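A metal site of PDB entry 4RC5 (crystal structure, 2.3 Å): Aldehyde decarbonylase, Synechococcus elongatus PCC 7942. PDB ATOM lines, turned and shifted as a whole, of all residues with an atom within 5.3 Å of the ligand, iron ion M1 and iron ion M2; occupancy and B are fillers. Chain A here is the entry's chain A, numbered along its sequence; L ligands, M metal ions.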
ATOM      1  N   TYR A  11      14.972  -4.193   5.441  1.00  0.00           N
ATOM      2  CA  TYR A  11      13.906  -4.137   4.459  1.00  0.00           C
ATOM      3  C   TYR A  11      13.843  -5.430   3.645  1.00  0.00           C
ATOM      4  O   TYR A  11      12.752  -5.901   3.267  1.00  0.00           O
ATOM      5  CB  TYR A  11      14.023  -2.907   3.527  1.00  0.00           C
ATOM      6  CG  TYR A  11      12.675  -2.466   3.057  1.00  0.00           C
ATOM      7  CD1 TYR A  11      11.870  -1.619   3.841  1.00  0.00           C
ATOM      8  CD2 TYR A  11      12.139  -2.936   1.868  1.00  0.00           C
ATOM      9  CE1 TYR A  11      10.617  -1.234   3.417  1.00  0.00           C
ATOM     10  CE2 TYR A  11      10.873  -2.547   1.445  1.00  0.00           C
ATOM     11  CZ  TYR A  11      10.130  -1.687   2.233  1.00  0.00           C
ATOM     12  OH  TYR A  11       8.863  -1.320   1.789  1.00  0.00           O
ATOM     13  N   ILE A  14      11.744  -7.677   5.962  1.00  0.00           N
ATOM     14  CA  ILE A  14      10.402  -7.154   6.213  1.00  0.00           C
ATOM     15  C   ILE A  14       9.576  -7.165   4.946  1.00  0.00           C
ATOM     16  O   ILE A  14       8.430  -7.591   4.951  1.00  0.00           O
ATOM     17  CB  ILE A  14      10.411  -5.706   6.760  1.00  0.00           C
ATOM     18  CG1 ILE A  14      11.000  -5.652   8.148  1.00  0.00           C
ATOM     19  CG2 ILE A  14       8.983  -5.108   6.764  1.00  0.00           C
ATOM     20  CD1 ILE A  14      10.145  -6.213   9.220  1.00  0.00           C
ATOM     21  N   ASN A  15      10.146  -6.676   3.863  1.00  0.00           N
ATOM     22  CA  ASN A  15       9.490  -6.723   2.564  1.00  0.00           C
ATOM     23  C   ASN A  15       9.129  -8.150   2.149  1.00  0.00           C
ATOM     24  O   ASN A  15       8.032  -8.409   1.645  1.00  0.00           O
ATOM     25  CB  ASN A  15      10.404  -6.120   1.528  1.00  0.00           C
ATOM     26  CG  ASN A  15       9.754  -6.028   0.167  1.00  0.00           C
ATOM     27  OD1 ASN A  15      10.351  -6.455  -0.828  1.00  0.00           O
ATOM     28  ND2 ASN A  15       8.560  -5.459   0.111  1.00  0.00           N
ATOM     29  N   ILE A  17       8.728 -10.735   4.216  1.00  0.00           N
ATOM     30  CA  ILE A  17       7.723 -11.237   5.148  1.00  0.00           C
ATOM     31  C   ILE A  17       6.339 -10.746   4.756  1.00  0.00           C
ATOM     32  O   ILE A  17       5.372 -11.532   4.746  1.00  0.00           O
ATOM     33  CB  ILE A  17       8.019 -10.802   6.595  1.00  0.00           C
ATOM     34  CG1 ILE A  17       9.045 -11.757   7.230  1.00  0.00           C
ATOM     35  CG2 ILE A  17       6.745 -10.770   7.411  1.00  0.00           C
ATOM     36  CD1 ILE A  17       9.686 -11.200   8.493  1.00  0.00           C
ATOM     37  N   VAL A  18       6.240  -9.466   4.427  1.00  0.00           N
ATOM     38  CA  VAL A  18       4.970  -8.873   4.028  1.00  0.00           C
ATOM     39  C   VAL A  18       4.459  -9.514   2.745  1.00  0.00           C
ATOM     40  O   VAL A  18       3.284  -9.810   2.610  1.00  0.00           O
ATOM     41  CB  VAL A  18       5.099  -7.350   3.841  1.00  0.00           C
ATOM     42  CG1 VAL A  18       4.203  -6.894   2.703  1.00  0.00           C
ATOM     43  CG2 VAL A  18       4.754  -6.619   5.149  1.00  0.00           C
ATOM     44  N   GLY A  21       3.030 -12.908   3.395  1.00  0.00           N
ATOM     45  CA  GLY A  21       1.730 -12.796   4.028  1.00  0.00           C
ATOM     46  C   GLY A  21       0.632 -12.570   3.030  1.00  0.00           C
ATOM     47  O   GLY A  21      -0.419 -13.206   3.101  1.00  0.00           O
ATOM     48  N   GLU A  22       0.867 -11.656   2.094  1.00  0.00           N
ATOM     49  CA  GLU A  22      -0.111 -11.343   1.058  1.00  0.00           C
ATOM     50  C   GLU A  22      -0.318 -12.544   0.146  1.00  0.00           C
ATOM     51  O   GLU A  22      -1.445 -12.889  -0.189  1.00  0.00           O
ATOM     52  CB  GLU A  22       0.336 -10.122   0.249  1.00  0.00           C
ATOM     53  CG  GLU A  22       0.319  -8.814   1.032  1.00  0.00           C
ATOM     54  CD  GLU A  22      -1.019  -8.525   1.650  1.00  0.00           C
ATOM     55  OE1 GLU A  22      -2.030  -9.116   1.215  1.00  0.00           O
ATOM     56  OE2 GLU A  22      -1.079  -7.694   2.589  1.00  0.00           O
ATOM     57  N   ALA A  25      -1.967 -15.319   2.104  1.00  0.00           N
ATOM     58  CA  ALA A  25      -3.364 -14.942   2.331  1.00  0.00           C
ATOM     59  C   ALA A  25      -4.219 -15.290   1.107  1.00  0.00           C
ATOM     60  O   ALA A  25      -5.369 -15.712   1.243  1.00  0.00           O
ATOM     61  CB  ALA A  25      -3.489 -13.473   2.664  1.00  0.00           C
ATOM     62  N   TYR A  29      -7.686 -17.540   1.554  1.00  0.00           N
ATOM     63  CA  TYR A  29      -9.035 -17.152   1.121  1.00  0.00           C
ATOM     64  C   TYR A  29      -9.623 -18.034   0.002  1.00  0.00           C
ATOM     65  O   TYR A  29     -10.803 -18.373   0.077  1.00  0.00           O
ATOM     66  CB  TYR A  29      -9.146 -15.672   0.817  1.00  0.00           C
ATOM     67  CG  TYR A  29      -9.084 -14.847   2.074  1.00  0.00           C
ATOM     68  CD1 TYR A  29      -9.997 -15.041   3.106  1.00  0.00           C
ATOM     69  CD2 TYR A  29      -8.107 -13.864   2.217  1.00  0.00           C
ATOM     70  CE1 TYR A  29      -9.934 -14.271   4.259  1.00  0.00           C
ATOM     71  CE2 TYR A  29      -8.026 -13.085   3.378  1.00  0.00           C
ATOM     72  CZ  TYR A  29      -8.940 -13.299   4.388  1.00  0.00           C
ATOM     73  OH  TYR A  29      -8.874 -12.537   5.520  1.00  0.00           O
ATOM     74  N   GLU A  50      -5.758  -9.865  -2.083  1.00  0.00           N
ATOM     75  CA  GLU A  50      -4.426 -10.237  -1.586  1.00  0.00           C
ATOM     76  C   GLU A  50      -3.356 -10.300  -2.713  1.00  0.00           C
ATOM     77  O   GLU A  50      -2.200  -9.884  -2.518  1.00  0.00           O
ATOM     78  CB  GLU A  50      -4.466 -11.555  -0.790  1.00  0.00           C
ATOM     79  CG  GLU A  50      -5.517 -11.605   0.308  1.00  0.00           C
ATOM     80  CD  GLU A  50      -5.216 -10.702   1.502  1.00  0.00           C
ATOM     81  OE1 GLU A  50      -4.414  -9.730   1.402  1.00  0.00           O
ATOM     82  OE2 GLU A  50      -5.800 -10.969   2.602  1.00  0.00           O
ATOM     83  N   HIS A  53      -2.130  -6.919  -3.372  1.00  0.00           N
ATOM     84  CA  HIS A  53      -1.233  -6.465  -2.316  1.00  0.00           C
ATOM     85  C   HIS A  53       0.132  -7.004  -2.520  1.00  0.00           C
ATOM     86  O   HIS A  53       1.104  -6.277  -2.313  1.00  0.00           O
ATOM     87  CB  HIS A  53      -1.690  -6.929  -0.932  1.00  0.00           C
ATOM     88  CG  HIS A  53      -3.074  -6.479  -0.580  1.00  0.00           C
ATOM     89  ND1 HIS A  53      -3.729  -6.987   0.452  1.00  0.00           N
ATOM     90  CD2 HIS A  53      -3.917  -5.551  -1.178  1.00  0.00           C
ATOM     91  CE1 HIS A  53      -4.953  -6.409   0.541  1.00  0.00           C
ATOM     92  NE2 HIS A  53      -5.062  -5.534  -0.469  1.00  0.00           N
ATOM     93  N   PHE A  57       3.562  -4.836  -2.868  1.00  0.00           N
ATOM     94  CA  PHE A  57       4.774  -4.924  -2.047  1.00  0.00           C
ATOM     95  C   PHE A  57       6.030  -5.423  -2.770  1.00  0.00           C
ATOM     96  O   PHE A  57       7.140  -5.030  -2.429  1.00  0.00           O
ATOM     97  CB  PHE A  57       4.512  -5.748  -0.779  1.00  0.00           C
ATOM     98  CG  PHE A  57       3.647  -5.010   0.208  1.00  0.00           C
ATOM     99  CD1 PHE A  57       4.054  -3.766   0.716  1.00  0.00           C
ATOM    100  CD2 PHE A  57       2.410  -5.527   0.590  1.00  0.00           C
ATOM    101  CE1 PHE A  57       3.250  -3.083   1.600  1.00  0.00           C
ATOM    102  CE2 PHE A  57       1.609  -4.846   1.504  1.00  0.00           C
ATOM    103  CZ  PHE A  57       2.022  -3.612   2.011  1.00  0.00           C
ATOM    104  N   PHE A  76       9.568 -17.811   8.580  1.00  0.00           N
ATOM    105  CA  PHE A  76       8.770 -16.919   9.498  1.00  0.00           C
ATOM    106  C   PHE A  76       7.328 -17.381   9.615  1.00  0.00           C
ATOM    107  O   PHE A  76       6.782 -17.475  10.732  1.00  0.00           O
ATOM    108  CB  PHE A  76       8.819 -15.486   8.940  1.00  0.00           C
ATOM    109  CG  PHE A  76       8.161 -14.424   9.812  1.00  0.00           C
ATOM    110  CD1 PHE A  76       8.823 -13.920  10.938  1.00  0.00           C
ATOM    111  CD2 PHE A  76       6.921 -13.877   9.447  1.00  0.00           C
ATOM    112  CE1 PHE A  76       8.243 -12.904  11.708  1.00  0.00           C
ATOM    113  CE2 PHE A  76       6.335 -12.867  10.237  1.00  0.00           C
ATOM    114  CZ  PHE A  76       7.015 -12.374  11.360  1.00  0.00           C
ATOM    115  N   PHE A  77       6.732 -17.705   8.473  1.00  0.00           N
ATOM    116  CA  PHE A  77       5.321 -18.050   8.372  1.00  0.00           C
ATOM    117  C   PHE A  77       4.978 -19.531   8.527  1.00  0.00           C
ATOM    118  O   PHE A  77       3.810 -19.877   8.711  1.00  0.00           O
ATOM    119  CB  PHE A  77       4.778 -17.591   7.002  1.00  0.00           C
ATOM    120  CG  PHE A  77       4.220 -16.218   7.026  1.00  0.00           C
ATOM    121  CD1 PHE A  77       2.947 -15.965   7.594  1.00  0.00           C
ATOM    122  CD2 PHE A  77       4.937 -15.158   6.507  1.00  0.00           C
ATOM    123  CE1 PHE A  77       2.437 -14.693   7.625  1.00  0.00           C
ATOM    124  CE2 PHE A  77       4.417 -13.869   6.541  1.00  0.00           C
ATOM    125  CZ  PHE A  77       3.172 -13.644   7.094  1.00  0.00           C
ATOM    126  N   GLN A 100      -6.533 -16.608   9.592  1.00  0.00           N
ATOM    127  CA  GLN A 100      -6.403 -15.648   8.560  1.00  0.00           C
ATOM    128  C   GLN A 100      -7.178 -14.363   8.725  1.00  0.00           C
ATOM    129  O   GLN A 100      -6.628 -13.313   8.689  1.00  0.00           O
ATOM    130  CB  GLN A 100      -6.655 -16.266   7.188  1.00  0.00           C
ATOM    131  CG  GLN A 100      -6.586 -15.251   6.086  1.00  0.00           C
ATOM    132  CD  GLN A 100      -5.215 -14.664   5.864  1.00  0.00           C
ATOM    133  OE1 GLN A 100      -4.254 -15.333   5.910  1.00  0.00           O
ATOM    134  NE2 GLN A 100      -5.147 -13.443   5.572  1.00  0.00           N
ATOM    135  N   ILE A 104      -4.299 -13.045  11.906  1.00  0.00           N
ATOM    136  CA  ILE A 104      -3.436 -12.517  10.851  1.00  0.00           C
ATOM    137  C   ILE A 104      -3.781 -11.171  10.263  1.00  0.00           C
ATOM    138  O   ILE A 104      -2.943 -10.355  10.179  1.00  0.00           O
ATOM    139  CB  ILE A 104      -3.204 -13.509   9.690  1.00  0.00           C
ATOM    140  CG1 ILE A 104      -2.254 -14.619  10.113  1.00  0.00           C
ATOM    141  CG2 ILE A 104      -2.625 -12.883   8.413  1.00  0.00           C
ATOM    142  CD1 ILE A 104      -2.026 -15.634   9.021  1.00  0.00           C
ATOM    143  N   GLU A 105      -4.976 -11.016   9.716  1.00  0.00           N
ATOM    144  CA  GLU A 105      -5.418  -9.707   9.248  1.00  0.00           C
ATOM    145  C   GLU A 105      -5.053  -8.639  10.274  1.00  0.00           C
ATOM    146  O   GLU A 105      -4.335  -7.690   9.970  1.00  0.00           O
ATOM    147  CB  GLU A 105      -6.926  -9.731   9.018  1.00  0.00           C
ATOM    148  CG  GLU A 105      -7.349 -10.476   7.767  1.00  0.00           C
ATOM    149  CD  GLU A 105      -6.800  -9.858   6.503  1.00  0.00           C
ATOM    150  OE1 GLU A 105      -6.799  -8.619   6.402  1.00  0.00           O
ATOM    151  OE2 GLU A 105      -6.362 -10.613   5.606  1.00  0.00           O
ATOM    152  N   PHE A 107      -2.968  -8.547  12.600  1.00  0.00           N
ATOM    153  CA  PHE A 107      -1.526  -8.355  12.677  1.00  0.00           C
ATOM    154  C   PHE A 107      -1.037  -7.398  11.583  1.00  0.00           C
ATOM    155  O   PHE A 107      -0.196  -6.544  11.833  1.00  0.00           O
ATOM    156  CB  PHE A 107      -0.804  -9.701  12.555  1.00  0.00           C
ATOM    157  CG  PHE A 107       0.673  -9.620  12.823  1.00  0.00           C
ATOM    158  CD1 PHE A 107       1.164  -8.840  13.856  1.00  0.00           C
ATOM    159  CD2 PHE A 107       1.573 -10.316  12.027  1.00  0.00           C
ATOM    160  CE1 PHE A 107       2.526  -8.765  14.106  1.00  0.00           C
ATOM    161  CE2 PHE A 107       2.935 -10.240  12.267  1.00  0.00           C
ATOM    162  CZ  PHE A 107       3.404  -9.463  13.302  1.00  0.00           C
ATOM    163  N   ALA A 108      -1.569  -7.561  10.383  1.00  0.00           N
ATOM    164  CA  ALA A 108      -1.188  -6.722   9.253  1.00  0.00           C
ATOM    165  C   ALA A 108      -1.706  -5.299   9.427  1.00  0.00           C
ATOM    166  O   ALA A 108      -1.078  -4.336   8.983  1.00  0.00           O
ATOM    167  CB  ALA A 108      -1.691  -7.320   7.951  1.00  0.00           C
ATOM    168  N   ALA A 111       0.581  -3.460  12.136  1.00  0.00           N
ATOM    169  CA  ALA A 111       1.939  -3.240  11.629  1.00  0.00           C
ATOM    170  C   ALA A 111       1.935  -2.291  10.441  1.00  0.00           C
ATOM    171  O   ALA A 111       2.737  -1.356  10.358  1.00  0.00           O
ATOM    172  CB  ALA A 111       2.564  -4.558  11.228  1.00  0.00           C
ATOM    173  N   TYR A 112       1.041  -2.537   9.500  1.00  0.00           N
ATOM    174  CA  TYR A 112       0.890  -1.647   8.375  1.00  0.00           C
ATOM    175  C   TYR A 112       0.605  -0.212   8.784  1.00  0.00           C
ATOM    176  O   TYR A 112       1.239   0.694   8.265  1.00  0.00           O
ATOM    177  CB  TYR A 112      -0.141  -2.177   7.391  1.00  0.00           C
ATOM    178  CG  TYR A 112       0.315  -3.426   6.691  1.00  0.00           C
ATOM    179  CD1 TYR A 112       1.426  -4.140   7.121  1.00  0.00           C
ATOM    180  CD2 TYR A 112      -0.400  -3.912   5.623  1.00  0.00           C
ATOM    181  CE1 TYR A 112       1.832  -5.298   6.483  1.00  0.00           C
ATOM    182  CE2 TYR A 112       0.008  -5.077   4.954  1.00  0.00           C
ATOM    183  CZ  TYR A 112       1.122  -5.755   5.396  1.00  0.00           C
ATOM    184  OH  TYR A 112       1.503  -6.928   4.760  1.00  0.00           O
ATOM    185  N   TYR A 115       3.730   1.205  10.026  1.00  0.00           N
ATOM    186  CA  TYR A 115       4.674   1.442   8.974  1.00  0.00           C
ATOM    187  C   TYR A 115       4.389   2.736   8.163  1.00  0.00           C
ATOM    188  O   TYR A 115       5.323   3.450   7.778  1.00  0.00           O
ATOM    189  CB  TYR A 115       4.785   0.216   8.074  1.00  0.00           C
ATOM    190  CG  TYR A 115       5.640   0.402   6.836  1.00  0.00           C
ATOM    191  CD1 TYR A 115       7.020   0.683   6.936  1.00  0.00           C
ATOM    192  CD2 TYR A 115       5.088   0.262   5.560  1.00  0.00           C
ATOM    193  CE1 TYR A 115       7.786   0.853   5.789  1.00  0.00           C
ATOM    194  CE2 TYR A 115       5.858   0.408   4.430  1.00  0.00           C
ATOM    195  CZ  TYR A 115       7.195   0.706   4.557  1.00  0.00           C
ATOM    196  OH  TYR A 115       7.944   0.866   3.411  1.00  0.00           O
ATOM    197  N   THR A 127       0.912   1.087   0.732  1.00  0.00           N
ATOM    198  CA  THR A 127       0.438   0.559   2.004  1.00  0.00           C
ATOM    199  C   THR A 127      -0.941   1.129   2.433  1.00  0.00           C
ATOM    200  O   THR A 127      -1.776   0.401   2.927  1.00  0.00           O
ATOM    201  CB  THR A 127       1.510   0.745   3.122  1.00  0.00           C
ATOM    202  OG1 THR A 127       2.771   0.192   2.657  1.00  0.00           O
ATOM    203  CG2 THR A 127       1.107   0.065   4.446  1.00  0.00           C
ATOM    204  N   GLU A 134      -7.653  -4.511   4.197  1.00  0.00           N
ATOM    205  CA  GLU A 134      -7.559  -5.337   5.383  1.00  0.00           C
ATOM    206  C   GLU A 134      -8.718  -5.149   6.327  1.00  0.00           C
ATOM    207  O   GLU A 134      -9.156  -6.116   6.941  1.00  0.00           O
ATOM    208  CB  GLU A 134      -6.200  -5.117   6.107  1.00  0.00           C
ATOM    209  CG  GLU A 134      -5.052  -5.330   5.133  1.00  0.00           C
ATOM    210  CD  GLU A 134      -3.693  -5.377   5.759  1.00  0.00           C
ATOM    211  OE1 GLU A 134      -3.403  -4.586   6.695  1.00  0.00           O
ATOM    212  OE2 GLU A 134      -2.886  -6.213   5.247  1.00  0.00           O
ATOM    213  N   HIS A 137     -11.359  -7.506   5.159  1.00  0.00           N
ATOM    214  CA  HIS A 137     -11.088  -8.909   5.419  1.00  0.00           C
ATOM    215  C   HIS A 137     -11.389  -9.275   6.843  1.00  0.00           C
ATOM    216  O   HIS A 137     -12.033 -10.278   7.084  1.00  0.00           O
ATOM    217  CB  HIS A 137      -9.602  -9.206   5.156  1.00  0.00           C
ATOM    218  CG  HIS A 137      -9.170  -8.918   3.753  1.00  0.00           C
ATOM    219  ND1 HIS A 137      -7.935  -9.188   3.319  1.00  0.00           N
ATOM    220  CD2 HIS A 137      -9.886  -8.408   2.649  1.00  0.00           C
ATOM    221  CE1 HIS A 137      -7.860  -8.840   2.002  1.00  0.00           C
ATOM    222  NE2 HIS A 137      -9.034  -8.367   1.614  1.00  0.00           N
ATOM    223  N   VAL A 174      10.221 -10.233  14.255  1.00  0.00           N
ATOM    224  CA  VAL A 174      10.382  -9.046  13.406  1.00  0.00           C
ATOM    225  C   VAL A 174      10.865  -7.817  14.176  1.00  0.00           C
ATOM    226  O   VAL A 174      11.237  -6.817  13.553  1.00  0.00           O
ATOM    227  CB  VAL A 174       9.102  -8.598  12.656  1.00  0.00           C
ATOM    228  CG1 VAL A 174       8.784  -9.507  11.514  1.00  0.00           C
ATOM    229  CG2 VAL A 174       7.917  -8.409  13.563  1.00  0.00           C
ATOM    230  N   LEU A 181      13.384   0.068  10.595  1.00  0.00           N
ATOM    231  CA  LEU A 181      12.452   0.752   9.689  1.00  0.00           C
ATOM    232  C   LEU A 181      11.648   1.896  10.351  1.00  0.00           C
ATOM    233  O   LEU A 181      10.815   2.545   9.704  1.00  0.00           O
ATOM    234  CB  LEU A 181      11.489  -0.278   9.078  1.00  0.00           C
ATOM    235  CG  LEU A 181      11.845  -0.931   7.753  1.00  0.00           C
ATOM    236  CD1 LEU A 181      13.129  -1.701   7.876  1.00  0.00           C
ATOM    237  CD2 LEU A 181      10.735  -1.853   7.267  1.00  0.00           C
ATOM    238  N   MET A 183       9.762   1.508  13.300  1.00  0.00           N
ATOM    239  CA  MET A 183       8.545   0.964  13.880  1.00  0.00           C
ATOM    240  C   MET A 183       8.829   0.395  15.282  1.00  0.00           C
ATOM    241  O   MET A 183       9.533  -0.597  15.398  1.00  0.00           O
ATOM    242  CB  MET A 183       7.981  -0.145  12.985  1.00  0.00           C
ATOM    243  CG  MET A 183       7.757   0.220  11.542  1.00  0.00           C
ATOM    244  SD  MET A 183       6.998  -1.120  10.574  1.00  0.00           S
ATOM    245  CE  MET A 183       8.341  -2.204  10.246  1.00  0.00           C
HETATM  246  C1  LIG L   1      -2.496 -10.215   4.527  1.00  0.00           C
HETATM  247  O1  LIG L   1      -3.724 -10.266   4.686  1.00  0.00           O
HETATM  248  C2  LIG L   1      -1.563 -10.824   5.579  1.00  0.00           C
HETATM  249  C3  LIG L   1      -0.210 -10.142   5.698  1.00  0.00           C
HETATM  250  C4  LIG L   1       0.378 -10.241   7.096  1.00  0.00           C
HETATM  251  C5  LIG L   1       1.880  -9.961   7.121  1.00  0.00           C
HETATM  252  C6  LIG L   1       2.257  -9.450   8.533  1.00  0.00           C
HETATM  253  C7  LIG L   1       3.726  -8.972   8.585  1.00  0.00           C
HETATM  254  C8  LIG L   1       3.944  -8.121   9.806  1.00  0.00           C
HETATM  255  C9  LIG L   1       5.429  -7.886  10.012  1.00  0.00           C
HETATM  256  C10 LIG L   1       5.886  -6.409   9.944  1.00  0.00           C
HETATM  257  C11 LIG L   1       4.962  -5.511   9.122  1.00  0.00           C
HETATM  258  C12 LIG L   1       5.629  -4.846   7.938  1.00  0.00           C
HETATM  259  C13 LIG L   1       5.005  -3.520   7.501  1.00  0.00           C
HETATM  260  C14 LIG L   1       5.845  -2.838   6.419  1.00  0.00           C
HETATM  261  C15 LIG L   1       5.566  -3.338   5.007  1.00  0.00           C
HETATM  262  C16 LIG L   1       6.687  -3.002   3.990  1.00  0.00           C
HETATM  263 FE    FE M   1      -5.766  -9.470   4.017  1.00  0.00          FE
HETATM  264 FE    FE M   2      -3.440  -8.300   2.380  1.00  0.00          FE
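The side-chain hydroxyl of Tyr 11 sits at hydrogen-bond distance from the side-chain hydroxyl of Tyr 115 (2.9 Å).
The side-chain hydroxyl (OH) of Tyr 29 sits close to the side-chain carboxylate (OE2) of Glu 105 (3.2 Å).
The backbone carbonyl oxygen (O) of Gln 100 lies within hydrogen-bond range of the backbone NH (N) of Glu 105 (3.0 Å).
The side-chain carboxylate (OE2) of Glu 22 sits close to the side-chain hydroxyl (OH) of Tyr 112 (3.5 Å).
Residues that only touch iron ion M2: Glu 134.
Within 4 Å of iron ion M2: Glu 22, Glu 50, His 53 and Glu 134.
OH of Tyr 11 touches C16 of the ligand, at 3.5 Å.
CG2 of Ile 14 touches C12 of the ligand, 3.6 Å away.
Ile 17 touches the ligand.
Val 18 touches the ligand.
Gly 21 touches the ligand.
CB of Ala 25 touches O1 of the ligand, 3.8 Å away.
Phe 77 touches the ligand (CZ to C5, 3.9 Å).
Gln 100 touches the ligand.
Ile 104 touches the ligand.
Phe 107 touches the ligand (CE2 to C8, 3.4 Å).
Ala 108 touches the ligand.
Ala 111 touches the ligand.
CD1 of Tyr 112 touches C13 of the ligand, 3.7 Å away.
CG of Tyr 115 touches C14 of the ligand, at 3.3 Å.
Hydrophobic or aromatic side chains that line the ligand: Ile 14, Ile 17, Val 18, Ala 25, Phe 77, Ile 104, Phe 107, Ala 108, Ala 111, Tyr 112 and Tyr 115.
Of the 28 residues printed, 3 come within 4 Å of iron ion M1.
The nearest printed residue that does not touch iron ion M1 is Tyr 29 (4.3 Å).
Iron ion M1 is bound by the side-chain carboxylate (OE2) of Glu 105 (2.0 Å), the side-chain carboxylate (OE2) of Glu 50 (2.1 Å), an oxygen (O1) of the ligand (2.3 Å) and a ring nitrogen (ND1) of His 137 (2.3 Å).
Iron ion M1 has four donor atoms within binding distance.
Slightly farther from iron ion M1 lies the side-chain carboxylate (OE1) of Glu 105 (2.7 Å).
Iron ion M2 is bound by OE1 of Glu 50, 2.0 Å away.
Iron ion M2 is bound by the side-chain carboxylate (OE1) of Glu 22.
Iron ion M2 is bound by a ring nitrogen (ND1) of His 53, at 2.4 Å.
Iron ion M2 is bound by OE2 of Glu 22, at 2.4 Å.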
